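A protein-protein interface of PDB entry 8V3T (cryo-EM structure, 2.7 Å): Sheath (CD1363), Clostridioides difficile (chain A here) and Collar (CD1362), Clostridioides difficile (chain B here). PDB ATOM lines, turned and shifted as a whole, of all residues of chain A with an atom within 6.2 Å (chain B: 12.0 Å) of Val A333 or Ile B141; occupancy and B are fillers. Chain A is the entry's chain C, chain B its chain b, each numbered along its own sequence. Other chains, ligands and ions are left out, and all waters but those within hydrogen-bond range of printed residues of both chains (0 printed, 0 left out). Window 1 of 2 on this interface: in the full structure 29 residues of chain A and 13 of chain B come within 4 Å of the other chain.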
ATOM      1  N   ARG A 254     -30.513 -27.597 -32.206  1.00  0.00           N
ATOM      2  CA  ARG A 254     -30.289 -28.010 -30.826  1.00  0.00           C
ATOM      3  C   ARG A 254     -29.011 -28.828 -30.670  1.00  0.00           C
ATOM      4  O   ARG A 254     -28.341 -28.729 -29.635  1.00  0.00           O
ATOM      5  CB  ARG A 254     -31.509 -28.786 -30.325  1.00  0.00           C
ATOM      6  CG  ARG A 254     -31.242 -29.781 -29.213  1.00  0.00           C
ATOM      7  CD  ARG A 254     -31.001 -29.062 -27.897  1.00  0.00           C
ATOM      8  NE  ARG A 254     -31.688 -27.778 -27.829  1.00  0.00           N
ATOM      9  CZ  ARG A 254     -31.756 -27.022 -26.741  1.00  0.00           C
ATOM     10  NH1 ARG A 254     -31.180 -27.389 -25.608  1.00  0.00           N
ATOM     11  NH2 ARG A 254     -32.415 -25.868 -26.792  1.00  0.00           N
ATOM     12  N   ILE A 257     -26.229 -26.440 -30.482  1.00  0.00           N
ATOM     13  CA  ILE A 257     -26.255 -25.788 -29.174  1.00  0.00           C
ATOM     14  C   ILE A 257     -25.615 -26.684 -28.117  1.00  0.00           C
ATOM     15  O   ILE A 257     -24.707 -26.265 -27.387  1.00  0.00           O
ATOM     16  CB  ILE A 257     -27.697 -25.409 -28.794  1.00  0.00           C
ATOM     17  CG1 ILE A 257     -28.135 -24.153 -29.550  1.00  0.00           C
ATOM     18  CG2 ILE A 257     -27.822 -25.208 -27.295  1.00  0.00           C
ATOM     19  CD1 ILE A 257     -29.566 -23.756 -29.292  1.00  0.00           C
ATOM     20  N   TYR A 261     -21.939 -25.660 -26.568  1.00  0.00           N
ATOM     21  CA  TYR A 261     -22.038 -24.590 -25.584  1.00  0.00           C
ATOM     22  C   TYR A 261     -22.590 -25.020 -24.233  1.00  0.00           C
ATOM     23  O   TYR A 261     -22.362 -24.315 -23.244  1.00  0.00           O
ATOM     24  CB  TYR A 261     -22.899 -23.445 -26.135  1.00  0.00           C
ATOM     25  CG  TYR A 261     -22.233 -22.682 -27.258  1.00  0.00           C
ATOM     26  CD1 TYR A 261     -22.195 -23.195 -28.545  1.00  0.00           C
ATOM     27  CD2 TYR A 261     -21.631 -21.454 -27.026  1.00  0.00           C
ATOM     28  CE1 TYR A 261     -21.584 -22.506 -29.571  1.00  0.00           C
ATOM     29  CE2 TYR A 261     -21.017 -20.757 -28.047  1.00  0.00           C
ATOM     30  CZ  TYR A 261     -20.996 -21.288 -29.316  1.00  0.00           C
ATOM     31  OH  TYR A 261     -20.387 -20.598 -30.337  1.00  0.00           O
ATOM     32  N   ILE A 262     -23.297 -26.141 -24.150  1.00  0.00           N
ATOM     33  CA  ILE A 262     -23.924 -26.543 -22.894  1.00  0.00           C
ATOM     34  C   ILE A 262     -22.860 -27.117 -21.966  1.00  0.00           C
ATOM     35  O   ILE A 262     -22.252 -28.151 -22.263  1.00  0.00           O
ATOM     36  CB  ILE A 262     -25.052 -27.556 -23.134  1.00  0.00           C
ATOM     37  CG1 ILE A 262     -26.255 -26.868 -23.779  1.00  0.00           C
ATOM     38  CG2 ILE A 262     -25.461 -28.215 -21.825  1.00  0.00           C
ATOM     39  CD1 ILE A 262     -27.066 -26.029 -22.818  1.00  0.00           C
ATOM     40  N   ASN A 267     -21.030 -18.100 -19.334  1.00  0.00           N
ATOM     41  CA  ASN A 267     -22.221 -17.338 -19.708  1.00  0.00           C
ATOM     42  C   ASN A 267     -21.885 -15.850 -19.694  1.00  0.00           C
ATOM     43  O   ASN A 267     -22.235 -15.101 -18.779  1.00  0.00           O
ATOM     44  CB  ASN A 267     -23.380 -17.663 -18.775  1.00  0.00           C
ATOM     45  CG  ASN A 267     -24.718 -17.254 -19.348  1.00  0.00           C
ATOM     46  OD1 ASN A 267     -24.886 -17.169 -20.562  1.00  0.00           O
ATOM     47  ND2 ASN A 267     -25.681 -16.996 -18.474  1.00  0.00           N
ATOM     48  N   LYS A 272     -22.445 -15.152 -26.004  1.00  0.00           N
ATOM     49  CA  LYS A 272     -23.801 -15.051 -26.528  1.00  0.00           C
ATOM     50  C   LYS A 272     -23.799 -14.499 -27.947  1.00  0.00           C
ATOM     51  O   LYS A 272     -24.534 -14.986 -28.814  1.00  0.00           O
ATOM     52  CB  LYS A 272     -24.649 -14.169 -25.613  1.00  0.00           C
ATOM     53  CG  LYS A 272     -24.962 -14.786 -24.265  1.00  0.00           C
ATOM     54  CD  LYS A 272     -25.735 -13.816 -23.392  1.00  0.00           C
ATOM     55  CE  LYS A 272     -26.072 -14.429 -22.046  1.00  0.00           C
ATOM     56  NZ  LYS A 272     -27.026 -13.586 -21.278  1.00  0.00           N
ATOM     57  N   LEU A 275     -22.654 -17.257 -30.303  1.00  0.00           N
ATOM     58  CA  LEU A 275     -23.728 -18.215 -30.546  1.00  0.00           C
ATOM     59  C   LEU A 275     -24.776 -17.644 -31.496  1.00  0.00           C
ATOM     60  O   LEU A 275     -25.273 -18.349 -32.388  1.00  0.00           O
ATOM     61  CB  LEU A 275     -24.361 -18.621 -29.216  1.00  0.00           C
ATOM     62  CG  LEU A 275     -25.455 -19.687 -29.204  1.00  0.00           C
ATOM     63  CD1 LEU A 275     -24.922 -21.021 -29.690  1.00  0.00           C
ATOM     64  CD2 LEU A 275     -26.029 -19.817 -27.806  1.00  0.00           C
ATOM     65  N   THR A 329     -27.330 -12.861 -16.500  1.00  0.00           N
ATOM     66  CA  THR A 329     -28.523 -13.681 -16.315  1.00  0.00           C
ATOM     67  C   THR A 329     -28.181 -15.056 -15.754  1.00  0.00           C
ATOM     68  O   THR A 329     -28.887 -16.031 -16.020  1.00  0.00           O
ATOM     69  CB  THR A 329     -29.297 -13.831 -17.625  1.00  0.00           C
ATOM     70  OG1 THR A 329     -28.468 -14.470 -18.603  1.00  0.00           O
ATOM     71  CG2 THR A 329     -29.739 -12.473 -18.149  1.00  0.00           C
ATOM     72  N   SER A 331     -27.100 -18.594 -15.358  1.00  0.00           N
ATOM     73  CA  SER A 331     -26.843 -19.703 -16.266  1.00  0.00           C
ATOM     74  C   SER A 331     -27.890 -19.820 -17.366  1.00  0.00           C
ATOM     75  O   SER A 331     -27.944 -20.847 -18.048  1.00  0.00           O
ATOM     76  CB  SER A 331     -26.764 -21.017 -15.487  1.00  0.00           C
ATOM     77  OG  SER A 331     -25.518 -21.145 -14.828  1.00  0.00           O
ATOM     78  N   LYS A 332     -28.719 -18.798 -17.558  1.00  0.00           N
ATOM     79  CA  LYS A 332     -29.817 -18.843 -18.513  1.00  0.00           C
ATOM     80  C   LYS A 332     -29.516 -17.963 -19.718  1.00  0.00           C
ATOM     81  O   LYS A 332     -29.027 -16.838 -19.573  1.00  0.00           O
ATOM     82  CB  LYS A 332     -31.126 -18.395 -17.859  1.00  0.00           C
ATOM     83  CG  LYS A 332     -31.467 -19.126 -16.573  1.00  0.00           C
ATOM     84  CD  LYS A 332     -32.164 -20.445 -16.857  1.00  0.00           C
ATOM     85  CE  LYS A 332     -33.070 -20.850 -15.706  1.00  0.00           C
ATOM     86  NZ  LYS A 332     -32.429 -20.628 -14.382  1.00  0.00           N
ATOM     87  N   VAL A 333     -29.812 -18.483 -20.907  1.00  0.00           N
ATOM     88  CA  VAL A 333     -29.690 -17.748 -22.160  1.00  0.00           C
ATOM     89  C   VAL A 333     -31.046 -17.759 -22.850  1.00  0.00           C
ATOM     90  O   VAL A 333     -31.634 -18.827 -23.050  1.00  0.00           O
ATOM     91  CB  VAL A 333     -28.609 -18.354 -23.075  1.00  0.00           C
ATOM     92  CG1 VAL A 333     -28.324 -17.424 -24.240  1.00  0.00           C
ATOM     93  CG2 VAL A 333     -27.340 -18.635 -22.291  1.00  0.00           C
ATOM     94  N   PHE A 334     -31.538 -16.577 -23.212  1.00  0.00           N
ATOM     95  CA  PHE A 334     -32.830 -16.426 -23.871  1.00  0.00           C
ATOM     96  C   PHE A 334     -32.615 -15.843 -25.260  1.00  0.00           C
ATOM     97  O   PHE A 334     -32.045 -14.756 -25.398  1.00  0.00           O
ATOM     98  CB  PHE A 334     -33.765 -15.534 -23.051  1.00  0.00           C
ATOM     99  CG  PHE A 334     -33.856 -15.921 -21.603  1.00  0.00           C
ATOM    100  CD1 PHE A 334     -34.692 -16.947 -21.199  1.00  0.00           C
ATOM    101  CD2 PHE A 334     -33.110 -15.258 -20.646  1.00  0.00           C
ATOM    102  CE1 PHE A 334     -34.779 -17.307 -19.870  1.00  0.00           C
ATOM    103  CE2 PHE A 334     -33.192 -15.613 -19.317  1.00  0.00           C
ATOM    104  CZ  PHE A 334     -34.028 -16.638 -18.928  1.00  0.00           C
ATOM    105  N   LEU A 335     -33.078 -16.560 -26.281  1.00  0.00           N
ATOM    106  CA  LEU A 335     -32.913 -16.157 -27.669  1.00  0.00           C
ATOM    107  C   LEU A 335     -34.238 -16.285 -28.404  1.00  0.00           C
ATOM    108  O   LEU A 335     -35.068 -17.136 -28.077  1.00  0.00           O
ATOM    109  CB  LEU A 335     -31.848 -17.005 -28.378  1.00  0.00           C
ATOM    110  CG  LEU A 335     -30.424 -16.944 -27.827  1.00  0.00           C
ATOM    111  CD1 LEU A 335     -29.495 -17.806 -28.662  1.00  0.00           C
ATOM    112  CD2 LEU A 335     -29.927 -15.511 -27.783  1.00  0.00           C
ATOM    113  N   TYR B 135     -17.894 -15.803 -14.544  1.00  0.00           N
ATOM    114  CA  TYR B 135     -19.191 -16.256 -15.014  1.00  0.00           C
ATOM    115  C   TYR B 135     -19.282 -17.768 -14.865  1.00  0.00           C
ATOM    116  O   TYR B 135     -18.279 -18.479 -14.977  1.00  0.00           O
ATOM    117  CB  TYR B 135     -19.425 -15.878 -16.482  1.00  0.00           C
ATOM    118  CG  TYR B 135     -19.344 -14.398 -16.778  1.00  0.00           C
ATOM    119  CD1 TYR B 135     -20.434 -13.567 -16.570  1.00  0.00           C
ATOM    120  CD2 TYR B 135     -18.181 -13.838 -17.287  1.00  0.00           C
ATOM    121  CE1 TYR B 135     -20.365 -12.216 -16.847  1.00  0.00           C
ATOM    122  CE2 TYR B 135     -18.103 -12.491 -17.568  1.00  0.00           C
ATOM    123  CZ  TYR B 135     -19.197 -11.685 -17.348  1.00  0.00           C
ATOM    124  OH  TYR B 135     -19.118 -10.341 -17.627  1.00  0.00           O
ATOM    125  N   GLU B 136     -20.490 -18.255 -14.609  1.00  0.00           N
ATOM    126  CA  GLU B 136     -20.737 -19.687 -14.611  1.00  0.00           C
ATOM    127  C   GLU B 136     -21.075 -20.157 -16.021  1.00  0.00           C
ATOM    128  O   GLU B 136     -21.443 -19.369 -16.894  1.00  0.00           O
ATOM    129  CB  GLU B 136     -21.860 -20.051 -13.640  1.00  0.00           C
ATOM    130  CG  GLU B 136     -23.104 -19.196 -13.764  1.00  0.00           C
ATOM    131  CD  GLU B 136     -23.062 -17.989 -12.852  1.00  0.00           C
ATOM    132  OE1 GLU B 136     -22.134 -17.905 -12.021  1.00  0.00           O
ATOM    133  OE2 GLU B 136     -23.955 -17.123 -12.962  1.00  0.00           O
ATOM    134  N   ASN B 137     -20.941 -21.462 -16.237  1.00  0.00           N
ATOM    135  CA  ASN B 137     -21.147 -22.022 -17.562  1.00  0.00           C
ATOM    136  C   ASN B 137     -22.627 -22.006 -17.932  1.00  0.00           C
ATOM    137  O   ASN B 137     -23.512 -21.972 -17.073  1.00  0.00           O
ATOM    138  CB  ASN B 137     -20.603 -23.448 -17.628  1.00  0.00           C
ATOM    139  CG  ASN B 137     -19.091 -23.495 -17.568  1.00  0.00           C
ATOM    140  OD1 ASN B 137     -18.479 -22.960 -16.646  1.00  0.00           O
ATOM    141  ND2 ASN B 137     -18.480 -24.136 -18.556  1.00  0.00           N
ATOM    142  N   MET B 138     -22.891 -22.026 -19.237  1.00  0.00           N
ATOM    143  CA  MET B 138     -24.263 -22.054 -19.723  1.00  0.00           C
ATOM    144  C   MET B 138     -24.874 -23.424 -19.460  1.00  0.00           C
ATOM    145  O   MET B 138     -24.372 -24.441 -19.948  1.00  0.00           O
ATOM    146  CB  MET B 138     -24.317 -21.726 -21.212  1.00  0.00           C
ATOM    147  CG  MET B 138     -23.484 -20.534 -21.642  1.00  0.00           C
ATOM    148  SD  MET B 138     -23.344 -20.436 -23.437  1.00  0.00           S
ATOM    149  CE  MET B 138     -22.900 -18.718 -23.657  1.00  0.00           C
ATOM    150  N   LYS B 139     -25.955 -23.451 -18.684  1.00  0.00           N
ATOM    151  CA  LYS B 139     -26.665 -24.686 -18.381  1.00  0.00           C
ATOM    152  C   LYS B 139     -27.940 -24.851 -19.194  1.00  0.00           C
ATOM    153  O   LYS B 139     -28.252 -25.963 -19.629  1.00  0.00           O
ATOM    154  CB  LYS B 139     -27.005 -24.750 -16.889  1.00  0.00           C
ATOM    155  CG  LYS B 139     -26.235 -25.808 -16.122  1.00  0.00           C
ATOM    156  CD  LYS B 139     -24.826 -25.346 -15.803  1.00  0.00           C
ATOM    157  CE  LYS B 139     -24.801 -24.501 -14.542  1.00  0.00           C
ATOM    158  NZ  LYS B 139     -25.360 -25.233 -13.373  1.00  0.00           N
ATOM    159  N   GLU B 140     -28.685 -23.770 -19.410  1.00  0.00           N
ATOM    160  CA  GLU B 140     -29.955 -23.817 -20.119  1.00  0.00           C
ATOM    161  C   GLU B 140     -29.963 -22.761 -21.211  1.00  0.00           C
ATOM    162  O   GLU B 140     -29.705 -21.583 -20.942  1.00  0.00           O
ATOM    163  CB  GLU B 140     -31.124 -23.595 -19.153  1.00  0.00           C
ATOM    164  CG  GLU B 140     -32.495 -23.761 -19.778  1.00  0.00           C
ATOM    165  CD  GLU B 140     -33.617 -23.537 -18.783  1.00  0.00           C
ATOM    166  OE1 GLU B 140     -33.533 -24.077 -17.659  1.00  0.00           O
ATOM    167  OE2 GLU B 140     -34.580 -22.818 -19.120  1.00  0.00           O
ATOM    168  N   ILE B 141     -30.258 -23.180 -22.439  1.00  0.00           N
ATOM    169  CA  ILE B 141     -30.365 -22.282 -23.584  1.00  0.00           C
ATOM    170  C   ILE B 141     -31.755 -22.465 -24.175  1.00  0.00           C
ATOM    171  O   ILE B 141     -32.067 -23.526 -24.729  1.00  0.00           O
ATOM    172  CB  ILE B 141     -29.277 -22.551 -24.632  1.00  0.00           C
ATOM    173  CG1 ILE B 141     -27.889 -22.428 -24.000  1.00  0.00           C
ATOM    174  CG2 ILE B 141     -29.418 -21.593 -25.802  1.00  0.00           C
ATOM    175  CD1 ILE B 141     -26.752 -22.517 -24.989  1.00  0.00           C
ATOM    176  N   ASN B 142     -32.588 -21.433 -24.064  1.00  0.00           N
ATOM    177  CA  ASN B 142     -33.970 -21.468 -24.530  1.00  0.00           C
ATOM    178  C   ASN B 142     -34.099 -20.594 -25.771  1.00  0.00           C
ATOM    179  O   ASN B 142     -34.011 -19.365 -25.681  1.00  0.00           O
ATOM    180  CB  ASN B 142     -34.925 -21.001 -23.434  1.00  0.00           C
ATOM    181  CG  ASN B 142     -34.744 -21.763 -22.140  1.00  0.00           C
ATOM    182  OD1 ASN B 142     -34.503 -22.969 -22.146  1.00  0.00           O
ATOM    183  ND2 ASN B 142     -34.856 -21.061 -21.019  1.00  0.00           N
ATOM    184  N   LEU B 143     -34.307 -21.226 -26.922  1.00  0.00           N
ATOM    185  CA  LEU B 143     -34.538 -20.524 -28.178  1.00  0.00           C
ATOM    186  C   LEU B 143     -35.914 -20.894 -28.713  1.00  0.00           C
ATOM    187  O   LEU B 143     -36.247 -22.079 -28.809  1.00  0.00           O
ATOM    188  CB  LEU B 143     -33.451 -20.861 -29.205  1.00  0.00           C
ATOM    189  CG  LEU B 143     -33.772 -20.719 -30.695  1.00  0.00           C
ATOM    190  CD1 LEU B 143     -32.595 -20.106 -31.425  1.00  0.00           C
ATOM    191  CD2 LEU B 143     -34.109 -22.068 -31.305  1.00  0.00           C
ATOM    192  N   ASN B 144     -36.710 -19.881 -29.050  1.00  0.00           N
ATOM    193  CA  ASN B 144     -38.022 -20.074 -29.655  1.00  0.00           C
ATOM    194  C   ASN B 144     -38.043 -19.420 -31.030  1.00  0.00           C
ATOM    195  O   ASN B 144     -37.727 -18.234 -31.166  1.00  0.00           O
ATOM    196  CB  ASN B 144     -39.136 -19.522 -28.759  1.00  0.00           C
ATOM    197  CG  ASN B 144     -38.982 -18.045 -28.463  1.00  0.00           C
ATOM    198  OD1 ASN B 144     -37.904 -17.475 -28.619  1.00  0.00           O
ATOM    199  ND2 ASN B 144     -40.069 -17.411 -28.040  1.00  0.00           N
ATOM    200  N   LEU B 145     -38.403 -20.196 -32.046  1.00  0.00           N
ATOM    201  CA  LEU B 145     -38.405 -19.735 -33.432  1.00  0.00           C
ATOM    202  C   LEU B 145     -39.845 -19.469 -33.873  1.00  0.00           C
ATOM    203  O   LEU B 145     -40.643 -20.392 -34.044  1.00  0.00           O
ATOM    204  CB  LEU B 145     -37.663 -20.733 -34.321  1.00  0.00           C
ATOM    205  CG  LEU B 145     -37.774 -22.256 -34.158  1.00  0.00           C
ATOM    206  CD1 LEU B 145     -39.054 -22.861 -34.703  1.00  0.00           C
ATOM    207  CD2 LEU B 145     -36.558 -22.927 -34.786  1.00  0.00           C
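Ile B141 touches Ile A257. O of Tyr A261 touches CB of Met B138, at 3.8 Å. CD1 of Ile A262 touches CG1 of Ile B141, at 3.9 Å. Tyr B135 touches Asn A267. Met B138 touches Asn A267. Leu A275 touches Ile B141 (CD2 to CD1, 3.97 Å). Glu B140 touches Lys A332 (O to CA, 3.7 Å). Val A333 touches Ile B141 (O to CA, 3.7 Å). CA of Phe A334 touches O of Asn B142 (3.6 Å). O of Leu A335 touches CA of Leu B143, at 3.4 Å.
OE2 of Glu B140 is in hydrogen-bond range of ND2 of Asn B142, at 2.6 Å. The side-chain hydroxyl of Thr A329 is in hydrogen-bond range of the backbone carbonyl oxygen of Lys A332, at 2.6 Å.
Of chain B, only Ile B141 (3.7 Å) comes within 4 Å of Ile A257. Ile A262 touches just these residues of chain B: Met B138, Lys B139 and Ile B141. Of chain B, only Tyr B135 (3.2 Å), Glu B136 (2.8 Å) and Met B138 (3.8 Å) come within 4 Å of Asn A267. No residue of chain B comes within 4 Å of Lys A272. No residue of chain B comes within 4 Å of Thr A329. Of chain B, only Glu B136, Asn B137, Lys B139 and Glu B140 come within 4 Å of Ser A331. Of chain B, only Glu B140, Ile B141 and Asn B142 come within 4 Å of Val A333. Of chain B, only Asn B142, Leu B143 and Asn B144 come within 4 Å of Leu A335. Printed residues of chain A within 4 Å of Tyr B135: Asn A267 (3.2 Å). Printed residues of chain A within 4 Å of Met B138: Tyr A261, Ile A262 and Asn A267. Of the printed residues of chain A, Asn B144 touches Leu A335 (2.9 Å). Leu B145 touches none of the printed residues of chain A. The nearest residue of chain B that does not touch Val A333 is Met B138 (4.3 Å).
The backbone carbonyl oxygen of Ile B141 is in hydrogen-bond range of the guanidinium group of Arg A254 (3.1 Å). O of Glu B140 lies within hydrogen-bond range of N of Val A333, at 3.1 Å. N of Leu A335 is in hydrogen-bond range of O of Asn B142 (3.0 Å). O of Ser A331 lies within hydrogen-bond range of N of Lys B139 (3.3 Å). The side-chain hydroxyl (OG) of Ser A331 lies within hydrogen-bond range of the backbone carbonyl oxygen (O) of Asn B137 (3.1 Å). N of Asn A267 lies within hydrogen-bond range of O of Glu B136, 2.8 Å away. The backbone carbonyl oxygen of Val A333 sits at hydrogen-bond distance from the backbone NH of Asn B142 (3.0 Å). The backbone carbonyl oxygen (O) of Leu A335 lies close to the side-chain amide oxygen (OD1) of Asn B144 (2.9 Å). The backbone carbonyl oxygen (O) of Ser A331 lies within hydrogen-bond range of the backbone NH (N) of Glu B140, 3.3 Å away.
Printed residues of chain B that touch a printed residue of chain A: Tyr B135, Glu B136, Asn B137, Met B138, Lys B139, Glu B140, Ile B141, Asn B142, Leu B143 and Asn B144. Hydrophobic or aromatic side chains of chain B within 4 Å of the printed part of chain A: Tyr B135, Met B138 and Ile B141. Among the printed residues, 22 pairs touch across the chains. Among the printed residues, no Asp or Glu carboxylate lies within 4 Å of a Lys or Arg side-chain nitrogen of the other chain.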
